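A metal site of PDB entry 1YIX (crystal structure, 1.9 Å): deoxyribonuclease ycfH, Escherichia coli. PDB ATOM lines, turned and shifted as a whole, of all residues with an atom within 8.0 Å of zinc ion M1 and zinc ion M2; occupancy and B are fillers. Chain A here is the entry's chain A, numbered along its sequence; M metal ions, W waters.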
ATOM      1  N   HIS A   7     -16.484  -6.829   4.411  1.00  0.00           N
ATOM      2  CA  HIS A   7     -15.317  -6.422   5.181  1.00  0.00           C
ATOM      3  C   HIS A   7     -15.082  -4.911   5.137  1.00  0.00           C
ATOM      4  O   HIS A   7     -14.568  -4.366   4.136  1.00  0.00           O
ATOM      5  CB  HIS A   7     -14.105  -7.139   4.603  1.00  0.00           C
ATOM      6  CG  HIS A   7     -12.881  -7.005   5.444  1.00  0.00           C
ATOM      7  ND1 HIS A   7     -12.437  -8.025   6.267  1.00  0.00           N
ATOM      8  CD2 HIS A   7     -12.010  -5.978   5.604  1.00  0.00           C
ATOM      9  CE1 HIS A   7     -11.345  -7.620   6.897  1.00  0.00           C
ATOM     10  NE2 HIS A   7     -11.068  -6.385   6.513  1.00  0.00           N
ATOM     11  N   CYS A   8     -15.465  -4.226   6.217  1.00  0.00           N
ATOM     12  CA  CYS A   8     -15.272  -2.780   6.318  1.00  0.00           C
ATOM     13  C   CYS A   8     -14.884  -2.359   7.726  1.00  0.00           C
ATOM     14  O   CYS A   8     -15.321  -2.959   8.722  1.00  0.00           O
ATOM     15  CB  CYS A   8     -16.532  -2.038   5.841  1.00  0.00           C
ATOM     16  SG  CYS A   8     -18.032  -2.376   6.802  1.00  0.00           S
ATOM     17  N   HIS A   9     -14.041  -1.331   7.815  1.00  0.00           N
ATOM     18  CA  HIS A   9     -13.588  -0.853   9.116  1.00  0.00           C
ATOM     19  C   HIS A   9     -14.430   0.377   9.460  1.00  0.00           C
ATOM     20  O   HIS A   9     -13.993   1.523   9.257  1.00  0.00           O
ATOM     21  CB  HIS A   9     -12.082  -0.530   9.068  1.00  0.00           C
ATOM     22  CG  HIS A   9     -11.201  -1.724   8.876  1.00  0.00           C
ATOM     23  ND1 HIS A   9     -10.846  -2.558   9.916  1.00  0.00           N
ATOM     24  CD2 HIS A   9     -10.676  -2.283   7.762  1.00  0.00           C
ATOM     25  CE1 HIS A   9     -10.142  -3.584   9.445  1.00  0.00           C
ATOM     26  NE2 HIS A   9     -10.028  -3.433   8.137  1.00  0.00           N
ATOM     27  N   VAL A  40     -15.377  -4.893  10.981  1.00  0.00           N
ATOM     28  CA  VAL A  40     -14.099  -5.459  11.413  1.00  0.00           C
ATOM     29  C   VAL A  40     -13.269  -4.645  12.406  1.00  0.00           C
ATOM     30  O   VAL A  40     -12.923  -3.497  12.137  1.00  0.00           O
ATOM     31  CB  VAL A  40     -13.180  -5.705  10.156  1.00  0.00           C
ATOM     32  CG1 VAL A  40     -11.876  -6.393  10.568  1.00  0.00           C
ATOM     33  CG2 VAL A  40     -13.924  -6.508   9.111  1.00  0.00           C
ATOM     34  N   ALA A  41     -12.910  -5.243  13.541  1.00  0.00           N
ATOM     35  CA  ALA A  41     -12.080  -4.578  14.555  1.00  0.00           C
ATOM     36  C   ALA A  41     -10.649  -5.084  14.344  1.00  0.00           C
ATOM     37  O   ALA A  41     -10.482  -6.210  13.862  1.00  0.00           O
ATOM     38  CB  ALA A  41     -12.573  -4.939  15.942  1.00  0.00           C
ATOM     39  N   THR A  42      -9.655  -4.274  14.698  1.00  0.00           N
ATOM     40  CA  THR A  42      -8.228  -4.629  14.544  1.00  0.00           C
ATOM     41  C   THR A  42      -7.512  -5.053  15.835  1.00  0.00           C
ATOM     42  O   THR A  42      -6.379  -5.569  15.769  1.00  0.00           O
ATOM     43  CB  THR A  42      -7.397  -3.472  13.947  1.00  0.00           C
ATOM     44  OG1 THR A  42      -7.487  -2.334  14.793  1.00  0.00           O
ATOM     45  CG2 THR A  42      -7.890  -3.097  12.572  1.00  0.00           C
ATOM     46  N   HIS A  67      -5.587  -8.078  14.438  1.00  0.00           N
ATOM     47  CA  HIS A  67      -4.904  -7.960  13.147  1.00  0.00           C
ATOM     48  C   HIS A  67      -3.420  -8.358  13.188  1.00  0.00           C
ATOM     49  O   HIS A  67      -2.741  -8.150  14.184  1.00  0.00           O
ATOM     50  CB  HIS A  67      -5.031  -6.496  12.719  1.00  0.00           C
ATOM     51  CG  HIS A  67      -4.630  -6.221  11.302  1.00  0.00           C
ATOM     52  ND1 HIS A  67      -5.552  -5.861  10.334  1.00  0.00           N
ATOM     53  CD2 HIS A  67      -3.413  -6.143  10.721  1.00  0.00           C
ATOM     54  CE1 HIS A  67      -4.908  -5.565   9.215  1.00  0.00           C
ATOM     55  NE2 HIS A  67      -3.611  -5.736   9.423  1.00  0.00           N
ATOM     56  N   PRO A  68      -2.898  -8.908  12.085  1.00  0.00           N
ATOM     57  CA  PRO A  68      -1.497  -9.322  11.960  1.00  0.00           C
ATOM     58  C   PRO A  68      -0.527  -8.197  12.229  1.00  0.00           C
ATOM     59  O   PRO A  68       0.565  -8.415  12.765  1.00  0.00           O
ATOM     60  CB  PRO A  68      -1.410  -9.782  10.507  1.00  0.00           C
ATOM     61  CG  PRO A  68      -2.726 -10.421  10.294  1.00  0.00           C
ATOM     62  CD  PRO A  68      -3.685  -9.427  10.956  1.00  0.00           C
ATOM     63  N   LEU A  69      -0.922  -6.978  11.869  1.00  0.00           N
ATOM     64  CA  LEU A  69      -0.045  -5.846  12.059  1.00  0.00           C
ATOM     65  C   LEU A  69      -0.141  -5.223  13.451  1.00  0.00           C
ATOM     66  O   LEU A  69       0.621  -4.306  13.783  1.00  0.00           O
ATOM     67  CB  LEU A  69      -0.325  -4.808  10.973  1.00  0.00           C
ATOM     68  CG  LEU A  69       0.072  -5.266   9.561  1.00  0.00           C
ATOM     69  CD1 LEU A  69      -0.015  -4.067   8.597  1.00  0.00           C
ATOM     70  CD2 LEU A  69       1.499  -5.811   9.573  1.00  0.00           C
ATOM     71  N   GLU A  94      -9.999  -9.645  11.941  1.00  0.00           N
ATOM     72  CA  GLU A  94      -9.199 -10.285  10.912  1.00  0.00           C
ATOM     73  C   GLU A  94      -7.851 -10.737  11.480  1.00  0.00           C
ATOM     74  O   GLU A  94      -7.209 -10.044  12.281  1.00  0.00           O
ATOM     75  CB  GLU A  94      -9.014  -9.371   9.683  1.00  0.00           C
ATOM     76  CG  GLU A  94      -8.196  -8.126   9.919  1.00  0.00           C
ATOM     77  CD  GLU A  94      -8.065  -7.323   8.643  1.00  0.00           C
ATOM     78  OE1 GLU A  94      -8.798  -6.341   8.498  1.00  0.00           O
ATOM     79  OE2 GLU A  94      -7.256  -7.714   7.790  1.00  0.00           O
ATOM     80  N   THR A  95      -7.470 -11.944  11.089  1.00  0.00           N
ATOM     81  CA  THR A  95      -6.225 -12.535  11.541  1.00  0.00           C
ATOM     82  C   THR A  95      -5.408 -12.791  10.268  1.00  0.00           C
ATOM     83  O   THR A  95      -5.676 -12.176   9.230  1.00  0.00           O
ATOM     84  CB  THR A  95      -6.513 -13.860  12.354  1.00  0.00           C
ATOM     85  OG1 THR A  95      -5.285 -14.396  12.860  1.00  0.00           O
ATOM     86  CG2 THR A  95      -7.225 -14.900  11.499  1.00  0.00           C
ATOM     87  N   ASP A  98       1.053 -10.782   7.828  1.00  0.00           N
ATOM     88  CA  ASP A  98       1.453  -9.678   6.988  1.00  0.00           C
ATOM     89  C   ASP A  98       2.947  -9.465   7.223  1.00  0.00           C
ATOM     90  O   ASP A  98       3.353  -9.007   8.296  1.00  0.00           O
ATOM     91  CB  ASP A  98       0.662  -8.418   7.348  1.00  0.00           C
ATOM     92  CG  ASP A  98       0.834  -7.325   6.349  1.00  0.00           C
ATOM     93  OD1 ASP A  98      -0.160  -6.640   6.044  1.00  0.00           O
ATOM     94  OD2 ASP A  98       1.976  -7.165   5.850  1.00  0.00           O
ATOM     95  N   ILE A 128     -11.541 -14.585   9.314  1.00  0.00           N
ATOM     96  CA  ILE A 128     -11.383 -13.634   8.203  1.00  0.00           C
ATOM     97  C   ILE A 128      -9.871 -13.509   8.142  1.00  0.00           C
ATOM     98  O   ILE A 128      -9.244 -13.053   9.087  1.00  0.00           O
ATOM     99  CB  ILE A 128     -12.013 -12.280   8.529  1.00  0.00           C
ATOM    100  CG1 ILE A 128     -13.536 -12.440   8.587  1.00  0.00           C
ATOM    101  CG2 ILE A 128     -11.666 -11.269   7.443  1.00  0.00           C
ATOM    102  CD1 ILE A 128     -14.270 -11.223   9.143  1.00  0.00           C
ATOM    103  N   VAL A 129      -9.298 -13.950   7.024  1.00  0.00           N
ATOM    104  CA  VAL A 129      -7.858 -13.997   6.851  1.00  0.00           C
ATOM    105  C   VAL A 129      -7.322 -12.919   5.952  1.00  0.00           C
ATOM    106  O   VAL A 129      -7.736 -12.804   4.795  1.00  0.00           O
ATOM    107  CB  VAL A 129      -7.403 -15.365   6.255  1.00  0.00           C
ATOM    108  CG1 VAL A 129      -5.864 -15.419   6.145  1.00  0.00           C
ATOM    109  CG2 VAL A 129      -7.926 -16.561   7.153  1.00  0.00           C
ATOM    110  N   HIS A 130      -6.381 -12.169   6.509  1.00  0.00           N
ATOM    111  CA  HIS A 130      -5.652 -11.115   5.832  1.00  0.00           C
ATOM    112  C   HIS A 130      -4.280 -11.745   5.609  1.00  0.00           C
ATOM    113  O   HIS A 130      -3.697 -12.277   6.549  1.00  0.00           O
ATOM    114  CB  HIS A 130      -5.456  -9.916   6.777  1.00  0.00           C
ATOM    115  CG  HIS A 130      -4.416  -8.936   6.312  1.00  0.00           C
ATOM    116  ND1 HIS A 130      -4.731  -7.757   5.668  1.00  0.00           N
ATOM    117  CD2 HIS A 130      -3.064  -8.974   6.389  1.00  0.00           C
ATOM    118  CE1 HIS A 130      -3.623  -7.116   5.370  1.00  0.00           C
ATOM    119  NE2 HIS A 130      -2.594  -7.825   5.790  1.00  0.00           N
ATOM    120  N   THR A 131      -3.761 -11.710   4.388  1.00  0.00           N
ATOM    121  CA  THR A 131      -2.429 -12.239   4.126  1.00  0.00           C
ATOM    122  C   THR A 131      -1.755 -11.280   3.141  1.00  0.00           C
ATOM    123  O   THR A 131      -2.430 -10.669   2.310  1.00  0.00           O
ATOM    124  CB  THR A 131      -2.459 -13.701   3.519  1.00  0.00           C
ATOM    125  OG1 THR A 131      -1.151 -14.282   3.603  1.00  0.00           O
ATOM    126  CG2 THR A 131      -2.864 -13.689   2.038  1.00  0.00           C
ATOM    127  N   HIS A 155      -9.917 -12.609   2.805  1.00  0.00           N
ATOM    128  CA  HIS A 155     -10.437 -11.253   2.566  1.00  0.00           C
ATOM    129  C   HIS A 155      -9.468 -10.380   1.745  1.00  0.00           C
ATOM    130  O   HIS A 155      -8.261 -10.520   1.874  1.00  0.00           O
ATOM    131  CB  HIS A 155     -10.807 -10.595   3.917  1.00  0.00           C
ATOM    132  CG  HIS A 155      -9.935  -9.438   4.293  1.00  0.00           C
ATOM    133  ND1 HIS A 155     -10.152  -8.167   3.826  1.00  0.00           N
ATOM    134  CD2 HIS A 155      -8.775  -9.386   4.993  1.00  0.00           C
ATOM    135  CE1 HIS A 155      -9.170  -7.372   4.208  1.00  0.00           C
ATOM    136  NE2 HIS A 155      -8.313  -8.091   4.917  1.00  0.00           N
ATOM    137  N   CYS A 156     -10.015  -9.465   0.933  1.00  0.00           N
ATOM    138  CA  CYS A 156      -9.193  -8.564   0.112  1.00  0.00           C
ATOM    139  C   CYS A 156      -8.061  -9.303  -0.618  1.00  0.00           C
ATOM    140  O   CYS A 156      -6.885  -8.922  -0.550  1.00  0.00           O
ATOM    141  CB  CYS A 156      -8.622  -7.452   0.998  1.00  0.00           C
ATOM    142  SG  CYS A 156      -7.859  -6.042   0.102  1.00  0.00           S
ATOM    143  N   GLU A 203     -16.096  -6.941  -1.048  1.00  0.00           N
ATOM    144  CA  GLU A 203     -15.949  -6.046   0.091  1.00  0.00           C
ATOM    145  C   GLU A 203     -15.292  -4.786  -0.388  1.00  0.00           C
ATOM    146  O   GLU A 203     -14.846  -4.707  -1.525  1.00  0.00           O
ATOM    147  CB  GLU A 203     -15.016  -6.665   1.092  1.00  0.00           C
ATOM    148  CG  GLU A 203     -13.586  -6.740   0.527  1.00  0.00           C
ATOM    149  CD  GLU A 203     -12.649  -7.536   1.392  1.00  0.00           C
ATOM    150  OE1 GLU A 203     -12.760  -8.791   1.399  1.00  0.00           O
ATOM    151  OE2 GLU A 203     -11.810  -6.908   2.069  1.00  0.00           O
ATOM    152  N   THR A 204     -15.164  -3.825   0.520  1.00  0.00           N
ATOM    153  CA  THR A 204     -14.473  -2.563   0.234  1.00  0.00           C
ATOM    154  C   THR A 204     -13.173  -2.471   1.052  1.00  0.00           C
ATOM    155  O   THR A 204     -12.198  -1.927   0.591  1.00  0.00           O
ATOM    156  CB  THR A 204     -15.331  -1.332   0.628  1.00  0.00           C
ATOM    157  OG1 THR A 204     -15.714  -1.427   2.023  1.00  0.00           O
ATOM    158  CG2 THR A 204     -16.592  -1.254  -0.234  1.00  0.00           C
ATOM    159  N   ASP A 205     -13.151  -3.066   2.253  1.00  0.00           N
ATOM    160  CA  ASP A 205     -12.037  -2.920   3.204  1.00  0.00           C
ATOM    161  C   ASP A 205     -11.949  -1.395   3.500  1.00  0.00           C
ATOM    162  O   ASP A 205     -10.860  -0.845   3.702  1.00  0.00           O
ATOM    163  CB  ASP A 205     -10.688  -3.435   2.668  1.00  0.00           C
ATOM    164  CG  ASP A 205      -9.697  -3.760   3.804  1.00  0.00           C
ATOM    165  OD1 ASP A 205     -10.111  -3.668   4.992  1.00  0.00           O
ATOM    166  OD2 ASP A 205      -8.518  -4.114   3.514  1.00  0.00           O
ATOM    167  N   SER A 206     -13.108  -0.751   3.519  1.00  0.00           N
ATOM    168  CA  SER A 206     -13.205   0.688   3.812  1.00  0.00           C
ATOM    169  C   SER A 206     -12.494   0.990   5.120  1.00  0.00           C
ATOM    170  O   SER A 206     -12.604   0.218   6.074  1.00  0.00           O
ATOM    171  CB  SER A 206     -14.661   1.135   3.937  1.00  0.00           C
ATOM    172  OG  SER A 206     -15.331   1.163   2.697  1.00  0.00           O
ATOM    173  N   PRO A 207     -11.853   2.161   5.202  1.00  0.00           N
ATOM    174  CA  PRO A 207     -11.780   3.240   4.201  1.00  0.00           C
ATOM    175  C   PRO A 207     -10.699   3.178   3.103  1.00  0.00           C
ATOM    176  O   PRO A 207     -10.525   4.137   2.338  1.00  0.00           O
ATOM    177  CB  PRO A 207     -11.602   4.476   5.079  1.00  0.00           C
ATOM    178  CG  PRO A 207     -10.623   3.970   6.105  1.00  0.00           C
ATOM    179  CD  PRO A 207     -11.224   2.595   6.476  1.00  0.00           C
ATOM    180  N   TYR A 208      -9.991   2.062   3.012  1.00  0.00           N
ATOM    181  CA  TYR A 208      -8.933   1.930   2.023  1.00  0.00           C
ATOM    182  C   TYR A 208      -9.386   1.392   0.668  1.00  0.00           C
ATOM    183  O   TYR A 208     -10.493   0.880   0.515  1.00  0.00           O
ATOM    184  CB  TYR A 208      -7.836   0.983   2.517  1.00  0.00           C
ATOM    185  CG  TYR A 208      -7.600   1.043   3.996  1.00  0.00           C
ATOM    186  CD1 TYR A 208      -7.190   2.231   4.604  1.00  0.00           C
ATOM    187  CD2 TYR A 208      -7.871  -0.061   4.811  1.00  0.00           C
ATOM    188  CE1 TYR A 208      -7.057   2.321   5.976  1.00  0.00           C
ATOM    189  CE2 TYR A 208      -7.749   0.010   6.186  1.00  0.00           C
ATOM    190  CZ  TYR A 208      -7.345   1.207   6.768  1.00  0.00           C
ATOM    191  OH  TYR A 208      -7.246   1.290   8.129  1.00  0.00           O
ATOM    192  N   LEU A 209      -8.498   1.518  -0.307  1.00  0.00           N
ATOM    193  CA  LEU A 209      -8.719   0.944  -1.628  1.00  0.00           C
ATOM    194  C   LEU A 209     -10.007   1.241  -2.381  1.00  0.00           C
ATOM    195  O   LEU A 209     -10.658   0.318  -2.889  1.00  0.00           O
ATOM    196  CB  LEU A 209      -8.561  -0.565  -1.499  1.00  0.00           C
ATOM    197  CG  LEU A 209      -7.330  -0.951  -0.684  1.00  0.00           C
ATOM    198  CD1 LEU A 209      -7.269  -2.461  -0.513  1.00  0.00           C
ATOM    199  CD2 LEU A 209      -6.077  -0.429  -1.406  1.00  0.00           C
HETATM  200 ZN    ZN M   1      -9.482  -5.006   6.918  1.00  0.00          ZN
HETATM  201 ZN    ZN M   2      -6.895  -6.953   5.910  1.00  0.00          ZN
HETATM  202  O   HOH W   1      -6.192  -5.917   3.706  1.00  0.00           O
HETATM  203  O   HOH W   2      -5.829  -3.959   7.062  1.00  0.00           O
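N of His 155 sits at hydrogen-bond distance from O of Val 129, at 3.0 Å. The backbone carbonyl oxygen (O) of Val 40 is in hydrogen-bond range of a ring nitrogen (ND1) of His 9 (3.2 Å). The backbone NH of His 130 lies within hydrogen-bond range of the backbone carbonyl oxygen of Thr 95 (2.8 Å). The backbone carbonyl oxygen (O) of Glu 94 sits close to the backbone NH (N) of His 67 (3.3 Å). The backbone carbonyl oxygen (O) of Ser 206 sits at hydrogen-bond distance from the backbone NH (N) of His 9 (2.7 Å). A ring nitrogen (ND1) of His 155 sits at hydrogen-bond distance from the side-chain carboxylate (OE2) of Glu 203 (2.7 Å). A ring nitrogen (NE2) of His 130 is in hydrogen-bond range of the side-chain carboxylate (OD1) of Asp 98 (2.7 Å). A ring nitrogen (ND1) of His 155 lies close to a ring nitrogen (ND1) of His 7 (3.3 Å).
Five residues have an atom within 4 Å of zinc ion M1: His 7, His 9, Glu 94, His 155 and Asp 205.
Within 4 Å of zinc ion M2: Glu 94, His 130 and His 155. The nearest printed residue that does not touch zinc ion M2 is Asp 205 (4.1 Å).
Zinc ion M1 is bound by NE2 of His 9, 2.1 Å away. NE2 of His 7 is bound to zinc ion M1, at 2.1 Å. Zinc ion M1 is bound by OE1 of Glu 94 (2.2 Å). Zinc ion M1 is bound by the side-chain carboxylate (OD1) of Asp 205 (2.4 Å). Zinc ion M1 has four donor atoms within binding distance.
Zinc ion M2 is bound by the side-chain carboxylate (OE2) of Glu 94 (2.1 Å), a ring nitrogen (NE2) of His 155 (2.1 Å), a ring nitrogen (ND1) of His 130 (2.3 Å) and water W1 (2.5 Å). Zinc ion M2 has four donor atoms within binding distance.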
